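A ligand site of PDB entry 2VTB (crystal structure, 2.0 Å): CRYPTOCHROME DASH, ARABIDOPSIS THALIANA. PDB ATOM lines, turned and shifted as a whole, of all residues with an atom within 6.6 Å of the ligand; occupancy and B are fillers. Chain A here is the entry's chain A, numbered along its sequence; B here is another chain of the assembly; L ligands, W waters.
ND2 of Asn 342 is in hydrogen-bond range of O6 of the ligand (2.8 Å). The side-chain carboxylate of Glu 418 lies within hydrogen-bond range of a nitrogen (N5) of the ligand, 3.1 Å away. A nitrogen (N7) of the ligand lies within hydrogen-bond range of the side-chain carboxylate of Asp 190 of chain B, 3.0 Å away. The side-chain carboxylate of Glu 149 sits close to a nitrogen (N3) of the ligand (3.4 Å). An oxygen (O1) of the ligand sits at hydrogen-bond distance from the backbone NH (N) of Glu 149, 2.9 Å away. OH of Tyr 424 lies within hydrogen-bond range of N1 of the ligand, at 2.8 Å. The backbone NH (N) of Ser 148 sits at hydrogen-bond distance from an oxygen (O1) of the ligand, 3.5 Å away. The side-chain amino group (NZ) of Lys 339 of chain B is in salt-bridge range of an oxygen (O5) of the ligand. NE2 of His 346 is in hydrogen-bond range of O2 of the ligand (2.9 Å). OE1 of Glu 150 is in hydrogen-bond range of N3 of the ligand.
OD2 of Asp 190 of chain B sits at hydrogen-bond distance from OG of Ser 148, 2.7 Å away. The side-chain amino group of Lys 339 of chain B sits at hydrogen-bond distance from the backbone carbonyl oxygen of Leu 191 of chain B, at 2.7 Å. OE2 of Glu 418 lies close to OH of Tyr 424, at 3.4 Å. The side-chain hydroxyl of Tyr 430 lies within hydrogen-bond range of the side-chain carboxylate of Glu 418 (2.8 Å). The side-chain amide nitrogen (ND2) of Asn 342 lies within hydrogen-bond range of the side-chain carboxylate (OD1) of Asp 190 of chain B, at 3.1 Å. ND2 of Asn 342 lies within hydrogen-bond range of O of Phe 189 of chain B (3.0 Å). OE1 of Glu 149 lies within salt-bridge range of NZ of Lys 90 (2.9 Å). OE2 of Glu 415 lies within hydrogen-bond range of N of His 84.
His 84 touches the ligand. Lys 90 touches the ligand (NZ to N1, 3.6 Å). Cys 147 touches the ligand (CB to O1, 3.5 Å). CD2 of Phe 345 touches N6 of the ligand, at 3.3 Å. Pro 426 touches the ligand. Tyr 430 touches the ligand. O of Phe 189 of chain B touches O6 of the ligand (3.6 Å). Asp 193 of chain B touches the ligand.
Water W6 bridges O5 of the ligand (3.0 Å) and N of Asp 193 of chain B (3.0 Å). Water W2 lies within hydrogen-bond range of the side-chain carboxylate of Glu 418 (2.8 Å), the backbone NH of His 84 (2.9 Å) and a nitrogen (N5) of the ligand (3.4 Å). Water W3 bridges OE2 of Glu 415 (2.9 Å) and OH of Tyr 430 (3.1 Å). Water W7 lies within hydrogen-bond range of the side-chain carboxylate (OE1) of Glu 149, the side-chain carboxylate (OE2) of Glu 150 and a nitrogen (N2) of the ligand.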
ATOM      1  N   THR A  83      21.272 -26.762  -4.342  1.00  0.00           N
ATOM      2  CA  THR A  83      22.095 -27.534  -3.401  1.00  0.00           C
ATOM      3  C   THR A  83      23.420 -27.983  -4.055  1.00  0.00           C
ATOM      4  O   THR A  83      23.548 -28.005  -5.279  1.00  0.00           O
ATOM      5  CB  THR A  83      21.328 -28.734  -2.799  1.00  0.00           C
ATOM      6  OG1 THR A  83      20.940 -29.641  -3.837  1.00  0.00           O
ATOM      7  CG2 THR A  83      20.079 -28.276  -2.035  1.00  0.00           C
ATOM      8  N   HIS A  84      24.376 -28.351  -3.208  1.00  0.00           N
ATOM      9  CA  HIS A  84      25.791 -28.472  -3.587  1.00  0.00           C
ATOM     10  C   HIS A  84      26.099 -29.562  -4.623  1.00  0.00           C
ATOM     11  O   HIS A  84      26.656 -29.277  -5.669  1.00  0.00           O
ATOM     12  CB  HIS A  84      26.637 -28.696  -2.335  1.00  0.00           C
ATOM     13  CG  HIS A  84      28.122 -28.641  -2.560  1.00  0.00           C
ATOM     14  ND1 HIS A  84      28.870 -27.506  -2.302  1.00  0.00           N
ATOM     15  CD2 HIS A  84      28.997 -29.577  -2.990  1.00  0.00           C
ATOM     16  CE1 HIS A  84      30.133 -27.745  -2.578  1.00  0.00           C
ATOM     17  NE2 HIS A  84      30.242 -28.986  -3.002  1.00  0.00           N
ATOM     18  N   PHE A  85      25.739 -30.809  -4.310  1.00  0.00           N
ATOM     19  CA  PHE A  85      26.118 -31.946  -5.151  1.00  0.00           C
ATOM     20  C   PHE A  85      25.065 -32.317  -6.208  1.00  0.00           C
ATOM     21  O   PHE A  85      25.436 -32.725  -7.304  1.00  0.00           O
ATOM     22  CB  PHE A  85      26.445 -33.187  -4.297  1.00  0.00           C
ATOM     23  CG  PHE A  85      27.694 -33.037  -3.471  1.00  0.00           C
ATOM     24  CD1 PHE A  85      28.944 -33.056  -4.083  1.00  0.00           C
ATOM     25  CD2 PHE A  85      27.635 -32.870  -2.096  1.00  0.00           C
ATOM     26  CE1 PHE A  85      30.114 -32.911  -3.332  1.00  0.00           C
ATOM     27  CE2 PHE A  85      28.792 -32.720  -1.328  1.00  0.00           C
ATOM     28  CZ  PHE A  85      30.038 -32.738  -1.948  1.00  0.00           C
ATOM     29  N   LYS A  90      17.844 -24.736  -3.352  1.00  0.00           N
ATOM     30  CA  LYS A  90      18.541 -24.451  -2.101  1.00  0.00           C
ATOM     31  C   LYS A  90      17.548 -24.239  -0.954  1.00  0.00           C
ATOM     32  O   LYS A  90      17.748 -24.748   0.150  1.00  0.00           O
ATOM     33  CB  LYS A  90      19.471 -23.243  -2.268  1.00  0.00           C
ATOM     34  CG  LYS A  90      20.253 -22.861  -1.002  1.00  0.00           C
ATOM     35  CD  LYS A  90      21.271 -23.927  -0.602  1.00  0.00           C
ATOM     36  CE  LYS A  90      22.247 -23.408   0.465  1.00  0.00           C
ATOM     37  NZ  LYS A  90      23.267 -24.443   0.846  1.00  0.00           N
ATOM     38  N   CYS A 147      29.379 -23.225   9.786  1.00  0.00           N
ATOM     39  CA  CYS A 147      29.662 -23.975   8.546  1.00  0.00           C
ATOM     40  C   CYS A 147      30.267 -23.134   7.420  1.00  0.00           C
ATOM     41  O   CYS A 147      30.114 -21.916   7.394  1.00  0.00           O
ATOM     42  CB  CYS A 147      28.415 -24.685   8.054  1.00  0.00           C
ATOM     43  SG  CYS A 147      27.827 -25.928   9.213  1.00  0.00           S
ATOM     44  N   SER A 148      30.934 -23.839   6.504  1.00  0.00           N
ATOM     45  CA  SER A 148      31.684 -23.279   5.376  1.00  0.00           C
ATOM     46  C   SER A 148      31.047 -22.079   4.676  1.00  0.00           C
ATOM     47  O   SER A 148      31.674 -21.031   4.546  1.00  0.00           O
ATOM     48  CB  SER A 148      31.924 -24.396   4.347  1.00  0.00           C
ATOM     49  OG  SER A 148      32.285 -23.867   3.078  1.00  0.00           O
ATOM     50  N   GLU A 149      29.818 -22.257   4.206  1.00  0.00           N
ATOM     51  CA  GLU A 149      29.158 -21.205   3.421  1.00  0.00           C
ATOM     52  C   GLU A 149      28.972 -19.929   4.242  1.00  0.00           C
ATOM     53  O   GLU A 149      29.231 -18.837   3.747  1.00  0.00           O
ATOM     54  CB  GLU A 149      27.817 -21.699   2.877  1.00  0.00           C
ATOM     55  CG  GLU A 149      27.981 -22.717   1.762  1.00  0.00           C
ATOM     56  CD  GLU A 149      26.686 -23.362   1.312  1.00  0.00           C
ATOM     57  OE1 GLU A 149      25.596 -22.994   1.811  1.00  0.00           O
ATOM     58  OE2 GLU A 149      26.766 -24.246   0.433  1.00  0.00           O
ATOM     59  N   GLU A 150      28.563 -20.097   5.499  1.00  0.00           N
ATOM     60  CA  GLU A 150      28.234 -18.979   6.359  1.00  0.00           C
ATOM     61  C   GLU A 150      29.492 -18.244   6.804  1.00  0.00           C
ATOM     62  O   GLU A 150      29.504 -17.019   6.878  1.00  0.00           O
ATOM     63  CB  GLU A 150      27.465 -19.448   7.607  1.00  0.00           C
ATOM     64  CG  GLU A 150      26.011 -19.792   7.370  1.00  0.00           C
ATOM     65  CD  GLU A 150      25.825 -20.993   6.468  1.00  0.00           C
ATOM     66  OE1 GLU A 150      26.490 -22.021   6.674  1.00  0.00           O
ATOM     67  OE2 GLU A 150      25.007 -20.889   5.523  1.00  0.00           O
ATOM     68  N   ASN A 342      34.302 -29.481   6.849  1.00  0.00           N
ATOM     69  CA  ASN A 342      33.643 -29.940   5.626  1.00  0.00           C
ATOM     70  C   ASN A 342      33.500 -31.442   5.481  1.00  0.00           C
ATOM     71  O   ASN A 342      32.730 -31.907   4.646  1.00  0.00           O
ATOM     72  CB  ASN A 342      34.328 -29.341   4.389  1.00  0.00           C
ATOM     73  CG  ASN A 342      34.143 -27.836   4.301  1.00  0.00           C
ATOM     74  OD1 ASN A 342      33.158 -27.282   4.805  1.00  0.00           O
ATOM     75  ND2 ASN A 342      35.092 -27.160   3.660  1.00  0.00           N
ATOM     76  N   SER A 343      34.216 -32.212   6.307  1.00  0.00           N
ATOM     77  CA  SER A 343      34.041 -33.670   6.317  1.00  0.00           C
ATOM     78  C   SER A 343      32.587 -34.048   6.700  1.00  0.00           C
ATOM     79  O   SER A 343      32.114 -35.143   6.382  1.00  0.00           O
ATOM     80  CB  SER A 343      35.063 -34.337   7.253  1.00  0.00           C
ATOM     81  OG  SER A 343      34.803 -34.008   8.599  1.00  0.00           O
ATOM     82  N   PHE A 345      30.098 -32.947   5.201  1.00  0.00           N
ATOM     83  CA  PHE A 345      29.383 -32.968   3.935  1.00  0.00           C
ATOM     84  C   PHE A 345      29.936 -33.968   2.926  1.00  0.00           C
ATOM     85  O   PHE A 345      29.337 -34.181   1.872  1.00  0.00           O
ATOM     86  CB  PHE A 345      29.370 -31.564   3.317  1.00  0.00           C
ATOM     87  CG  PHE A 345      28.946 -30.478   4.275  1.00  0.00           C
ATOM     88  CD1 PHE A 345      27.654 -30.458   4.806  1.00  0.00           C
ATOM     89  CD2 PHE A 345      29.834 -29.475   4.650  1.00  0.00           C
ATOM     90  CE1 PHE A 345      27.263 -29.475   5.702  1.00  0.00           C
ATOM     91  CE2 PHE A 345      29.442 -28.481   5.536  1.00  0.00           C
ATOM     92  CZ  PHE A 345      28.154 -28.475   6.064  1.00  0.00           C
ATOM     93  N   HIS A 346      31.076 -34.584   3.221  1.00  0.00           N
ATOM     94  CA  HIS A 346      31.733 -35.490   2.286  1.00  0.00           C
ATOM     95  C   HIS A 346      31.139 -36.886   2.392  1.00  0.00           C
ATOM     96  O   HIS A 346      30.637 -37.278   3.444  1.00  0.00           O
ATOM     97  CB  HIS A 346      33.243 -35.522   2.519  1.00  0.00           C
ATOM     98  CG  HIS A 346      33.924 -34.226   2.225  1.00  0.00           C
ATOM     99  ND1 HIS A 346      35.121 -33.855   2.823  1.00  0.00           N
ATOM    100  CD2 HIS A 346      33.584 -33.203   1.406  1.00  0.00           C
ATOM    101  CE1 HIS A 346      35.483 -32.670   2.379  1.00  0.00           C
ATOM    102  NE2 HIS A 346      34.576 -32.247   1.514  1.00  0.00           N
ATOM    103  N   GLU A 415      20.392 -33.664   1.029  1.00  0.00           N
ATOM    104  CA  GLU A 415      20.137 -32.458   0.225  1.00  0.00           C
ATOM    105  C   GLU A 415      18.658 -32.237  -0.056  1.00  0.00           C
ATOM    106  O   GLU A 415      18.210 -31.104  -0.163  1.00  0.00           O
ATOM    107  CB  GLU A 415      20.934 -32.466  -1.094  1.00  0.00           C
ATOM    108  CG  GLU A 415      22.429 -32.141  -0.901  1.00  0.00           C
ATOM    109  CD  GLU A 415      23.190 -31.843  -2.188  1.00  0.00           C
ATOM    110  OE1 GLU A 415      22.592 -31.781  -3.299  1.00  0.00           O
ATOM    111  OE2 GLU A 415      24.421 -31.656  -2.063  1.00  0.00           O
ATOM    112  N   GLU A 418      17.406 -30.757   2.995  1.00  0.00           N
ATOM    113  CA  GLU A 418      17.828 -29.345   2.940  1.00  0.00           C
ATOM    114  C   GLU A 418      16.843 -28.490   2.131  1.00  0.00           C
ATOM    115  O   GLU A 418      16.543 -27.371   2.520  1.00  0.00           O
ATOM    116  CB  GLU A 418      19.241 -29.189   2.360  1.00  0.00           C
ATOM    117  CG  GLU A 418      19.680 -27.722   2.248  1.00  0.00           C
ATOM    118  CD  GLU A 418      21.174 -27.524   1.969  1.00  0.00           C
ATOM    119  OE1 GLU A 418      21.908 -28.520   1.755  1.00  0.00           O
ATOM    120  OE2 GLU A 418      21.583 -26.341   1.937  1.00  0.00           O
ATOM    121  N   TYR A 424      15.400 -26.883   8.622  1.00  0.00           N
ATOM    122  CA  TYR A 424      16.727 -27.173   8.097  1.00  0.00           C
ATOM    123  C   TYR A 424      17.826 -26.370   8.805  1.00  0.00           C
ATOM    124  O   TYR A 424      17.765 -25.148   8.902  1.00  0.00           O
ATOM    125  CB  TYR A 424      16.848 -26.911   6.588  1.00  0.00           C
ATOM    126  CG  TYR A 424      18.289 -27.014   6.153  1.00  0.00           C
ATOM    127  CD1 TYR A 424      18.941 -28.242   6.174  1.00  0.00           C
ATOM    128  CD2 TYR A 424      19.023 -25.882   5.793  1.00  0.00           C
ATOM    129  CE1 TYR A 424      20.282 -28.355   5.809  1.00  0.00           C
ATOM    130  CE2 TYR A 424      20.372 -25.987   5.436  1.00  0.00           C
ATOM    131  CZ  TYR A 424      20.987 -27.224   5.440  1.00  0.00           C
ATOM    132  OH  TYR A 424      22.316 -27.353   5.089  1.00  0.00           O
ATOM    133  N   ASP A 425      18.840 -27.109   9.257  1.00  0.00           N
ATOM    134  CA  ASP A 425      20.010 -26.572   9.943  1.00  0.00           C
ATOM    135  C   ASP A 425      21.176 -27.462   9.480  1.00  0.00           C
ATOM    136  O   ASP A 425      21.086 -28.684   9.644  1.00  0.00           O
ATOM    137  CB  ASP A 425      19.763 -26.688  11.464  1.00  0.00           C
ATOM    138  CG  ASP A 425      20.941 -26.262  12.300  1.00  0.00           C
ATOM    139  OD1 ASP A 425      20.755 -25.330  13.125  1.00  0.00           O
ATOM    140  OD2 ASP A 425      22.017 -26.878  12.202  1.00  0.00           O
ATOM    141  N   PRO A 426      22.241 -26.892   8.893  1.00  0.00           N
ATOM    142  CA  PRO A 426      23.291 -27.763   8.354  1.00  0.00           C
ATOM    143  C   PRO A 426      23.895 -28.702   9.402  1.00  0.00           C
ATOM    144  O   PRO A 426      24.182 -29.855   9.082  1.00  0.00           O
ATOM    145  CB  PRO A 426      24.352 -26.779   7.841  1.00  0.00           C
ATOM    146  CG  PRO A 426      24.047 -25.480   8.488  1.00  0.00           C
ATOM    147  CD  PRO A 426      22.570 -25.462   8.717  1.00  0.00           C
ATOM    148  N   TYR A 430      23.077 -32.568   8.517  1.00  0.00           N
ATOM    149  CA  TYR A 430      24.219 -33.381   8.107  1.00  0.00           C
ATOM    150  C   TYR A 430      24.807 -34.200   9.255  1.00  0.00           C
ATOM    151  O   TYR A 430      25.294 -35.315   9.056  1.00  0.00           O
ATOM    152  CB  TYR A 430      25.255 -32.520   7.369  1.00  0.00           C
ATOM    153  CG  TYR A 430      24.711 -32.087   6.019  1.00  0.00           C
ATOM    154  CD1 TYR A 430      24.901 -32.879   4.886  1.00  0.00           C
ATOM    155  CD2 TYR A 430      23.963 -30.924   5.892  1.00  0.00           C
ATOM    156  CE1 TYR A 430      24.395 -32.506   3.656  1.00  0.00           C
ATOM    157  CE2 TYR A 430      23.441 -30.546   4.648  1.00  0.00           C
ATOM    158  CZ  TYR A 430      23.668 -31.340   3.542  1.00  0.00           C
ATOM    159  OH  TYR A 430      23.167 -30.980   2.308  1.00  0.00           O
ATOM    160  N   PHE B 189      38.583 -23.282   6.735  1.00  0.00           N
ATOM    161  CA  PHE B 189      37.851 -24.537   6.534  1.00  0.00           C
ATOM    162  C   PHE B 189      37.862 -24.992   5.069  1.00  0.00           C
ATOM    163  O   PHE B 189      37.697 -26.172   4.784  1.00  0.00           O
ATOM    164  CB  PHE B 189      36.405 -24.406   7.052  1.00  0.00           C
ATOM    165  CG  PHE B 189      36.255 -24.745   8.522  1.00  0.00           C
ATOM    166  CD1 PHE B 189      37.302 -24.555   9.414  1.00  0.00           C
ATOM    167  CD2 PHE B 189      35.040 -25.221   9.001  1.00  0.00           C
ATOM    168  CE1 PHE B 189      37.148 -24.869  10.766  1.00  0.00           C
ATOM    169  CE2 PHE B 189      34.878 -25.543  10.345  1.00  0.00           C
ATOM    170  CZ  PHE B 189      35.926 -25.365  11.225  1.00  0.00           C
ATOM    171  N   ASP B 190      38.064 -24.034   4.162  1.00  0.00           N
ATOM    172  CA  ASP B 190      38.161 -24.327   2.731  1.00  0.00           C
ATOM    173  C   ASP B 190      39.586 -24.130   2.185  1.00  0.00           C
ATOM    174  O   ASP B 190      39.775 -23.905   0.994  1.00  0.00           O
ATOM    175  CB  ASP B 190      37.159 -23.442   1.956  1.00  0.00           C
ATOM    176  CG  ASP B 190      35.728 -23.979   2.030  1.00  0.00           C
ATOM    177  OD1 ASP B 190      35.467 -25.054   1.458  1.00  0.00           O
ATOM    178  OD2 ASP B 190      34.866 -23.316   2.633  1.00  0.00           O
ATOM    179  N   LEU B 191      40.587 -24.246   3.052  1.00  0.00           N
ATOM    180  CA  LEU B 191      41.994 -24.152   2.624  1.00  0.00           C
ATOM    181  C   LEU B 191      42.273 -25.232   1.570  1.00  0.00           C
ATOM    182  O   LEU B 191      41.914 -26.390   1.770  1.00  0.00           O
ATOM    183  CB  LEU B 191      42.927 -24.349   3.815  1.00  0.00           C
ATOM    184  CG  LEU B 191      44.397 -23.988   3.590  1.00  0.00           C
ATOM    185  CD1 LEU B 191      44.554 -22.475   3.662  1.00  0.00           C
ATOM    186  CD2 LEU B 191      45.301 -24.700   4.611  1.00  0.00           C
ATOM    187  N   PRO B 192      42.901 -24.862   0.432  1.00  0.00           N
ATOM    188  CA  PRO B 192      43.192 -25.910  -0.557  1.00  0.00           C
ATOM    189  C   PRO B 192      44.037 -27.047   0.029  1.00  0.00           C
ATOM    190  O   PRO B 192      44.952 -26.792   0.804  1.00  0.00           O
ATOM    191  CB  PRO B 192      43.966 -25.164  -1.652  1.00  0.00           C
ATOM    192  CG  PRO B 192      43.543 -23.723  -1.500  1.00  0.00           C
ATOM    193  CD  PRO B 192      43.345 -23.527  -0.022  1.00  0.00           C
ATOM    194  N   ASP B 193      43.714 -28.289  -0.344  1.00  0.00           N
ATOM    195  CA  ASP B 193      44.467 -29.453   0.115  1.00  0.00           C
ATOM    196  C   ASP B 193      45.774 -29.654  -0.634  1.00  0.00           C
ATOM    197  O   ASP B 193      46.536 -30.550  -0.304  1.00  0.00           O
ATOM    198  CB  ASP B 193      43.595 -30.733   0.034  1.00  0.00           C
ATOM    199  CG  ASP B 193      42.572 -30.821   1.160  1.00  0.00           C
ATOM    200  OD1 ASP B 193      42.779 -30.219   2.236  1.00  0.00           O
ATOM    201  OD2 ASP B 193      41.544 -31.500   0.968  1.00  0.00           O
ATOM    202  N   LYS B 339      42.475 -26.359   9.812  1.00  0.00           N
ATOM    203  CA  LYS B 339      41.579 -27.173   8.995  1.00  0.00           C
ATOM    204  C   LYS B 339      41.538 -28.618   9.478  1.00  0.00           C
ATOM    205  O   LYS B 339      40.469 -29.223   9.515  1.00  0.00           O
ATOM    206  CB  LYS B 339      41.970 -27.141   7.519  1.00  0.00           C
ATOM    207  CG  LYS B 339      40.899 -27.690   6.594  1.00  0.00           C
ATOM    208  CD  LYS B 339      41.373 -27.816   5.170  1.00  0.00           C
ATOM    209  CE  LYS B 339      40.326 -28.499   4.307  1.00  0.00           C
ATOM    210  NZ  LYS B 339      40.695 -28.585   2.882  1.00  0.00           N
HETATM  211  N1  LIG L   1      24.268 -25.540   4.116  1.00  0.00           N
HETATM  212  C1  LIG L   1      24.701 -24.490   4.826  1.00  0.00           C
HETATM  213  N2  LIG L   1      23.775 -23.706   5.418  1.00  0.00           N
HETATM  214  N3  LIG L   1      26.017 -24.195   4.979  1.00  0.00           N
HETATM  215  C2  LIG L   1      26.994 -24.943   4.410  1.00  0.00           C
HETATM  216  O1  LIG L   1      28.212 -24.666   4.529  1.00  0.00           O
HETATM  217  C3  LIG L   1      26.569 -26.090   3.585  1.00  0.00           C
HETATM  218  N4  LIG L   1      27.422 -26.999   2.956  1.00  0.00           N
HETATM  219  C4  LIG L   1      26.821 -27.545   1.729  1.00  0.00           C
HETATM  220  C5  LIG L   1      25.597 -28.343   2.152  1.00  0.00           C
HETATM  221  N5  LIG L   1      24.665 -27.415   2.776  1.00  0.00           N
HETATM  222  C6  LIG L   1      25.105 -26.356   3.495  1.00  0.00           C
HETATM  223  C7  LIG L   1      27.966 -28.320   1.088  1.00  0.00           C
HETATM  224  N6  LIG L   1      29.131 -27.902   1.885  1.00  0.00           N
HETATM  225  C8  LIG L   1      28.780 -26.647   2.571  1.00  0.00           C
HETATM  226  C9  LIG L   1      33.123 -28.499   0.618  1.00  0.00           C
HETATM  227  C10 LIG L   1      32.759 -27.327   1.277  1.00  0.00           C
HETATM  228  C11 LIG L   1      31.450 -27.105   1.685  1.00  0.00           C
HETATM  229  C12 LIG L   1      30.457 -28.070   1.421  1.00  0.00           C
HETATM  230  C13 LIG L   1      30.818 -29.261   0.793  1.00  0.00           C
HETATM  231  C14 LIG L   1      32.138 -29.476   0.381  1.00  0.00           C
HETATM  232  C15 LIG L   1      34.547 -28.745   0.197  1.00  0.00           C
HETATM  233  O2  LIG L   1      34.863 -29.895  -0.070  1.00  0.00           O
HETATM  234  N7  LIG L   1      35.466 -27.780   0.184  1.00  0.00           N
HETATM  235  C16 LIG L   1      36.884 -28.064  -0.037  1.00  0.00           C
HETATM  236  C17 LIG L   1      37.651 -26.796  -0.420  1.00  0.00           C
HETATM  237  C18 LIG L   1      37.095 -26.070  -1.639  1.00  0.00           C
HETATM  238  C19 LIG L   1      36.949 -26.973  -2.837  1.00  0.00           C
HETATM  239  O3  LIG L   1      35.786 -27.226  -3.237  1.00  0.00           O
HETATM  240  O4  LIG L   1      37.979 -27.449  -3.365  1.00  0.00           O
HETATM  241  C20 LIG L   1      37.564 -28.668   1.159  1.00  0.00           C
HETATM  242  O5  LIG L   1      38.702 -29.163   0.990  1.00  0.00           O
HETATM  243  O6  LIG L   1      37.013 -28.649   2.295  1.00  0.00           O
HETATM  244  O   HOH W   1      37.734 -30.909   3.542  1.00  0.00           O
HETATM  245  O   HOH W   2      23.668 -27.979  -0.416  1.00  0.00           O
HETATM  246  O   HOH W   3      25.663 -31.304   0.484  1.00  0.00           O
HETATM  247  O   HOH W   4      21.084 -22.585   6.628  1.00  0.00           O
HETATM  248  O   HOH W   5      20.874 -22.690   3.962  1.00  0.00           O
HETATM  249  O   HOH W   6      40.784 -28.706  -1.055  1.00  0.00           O
HETATM  250  O   HOH W   7      23.830 -21.358   2.896  1.00  0.00           O
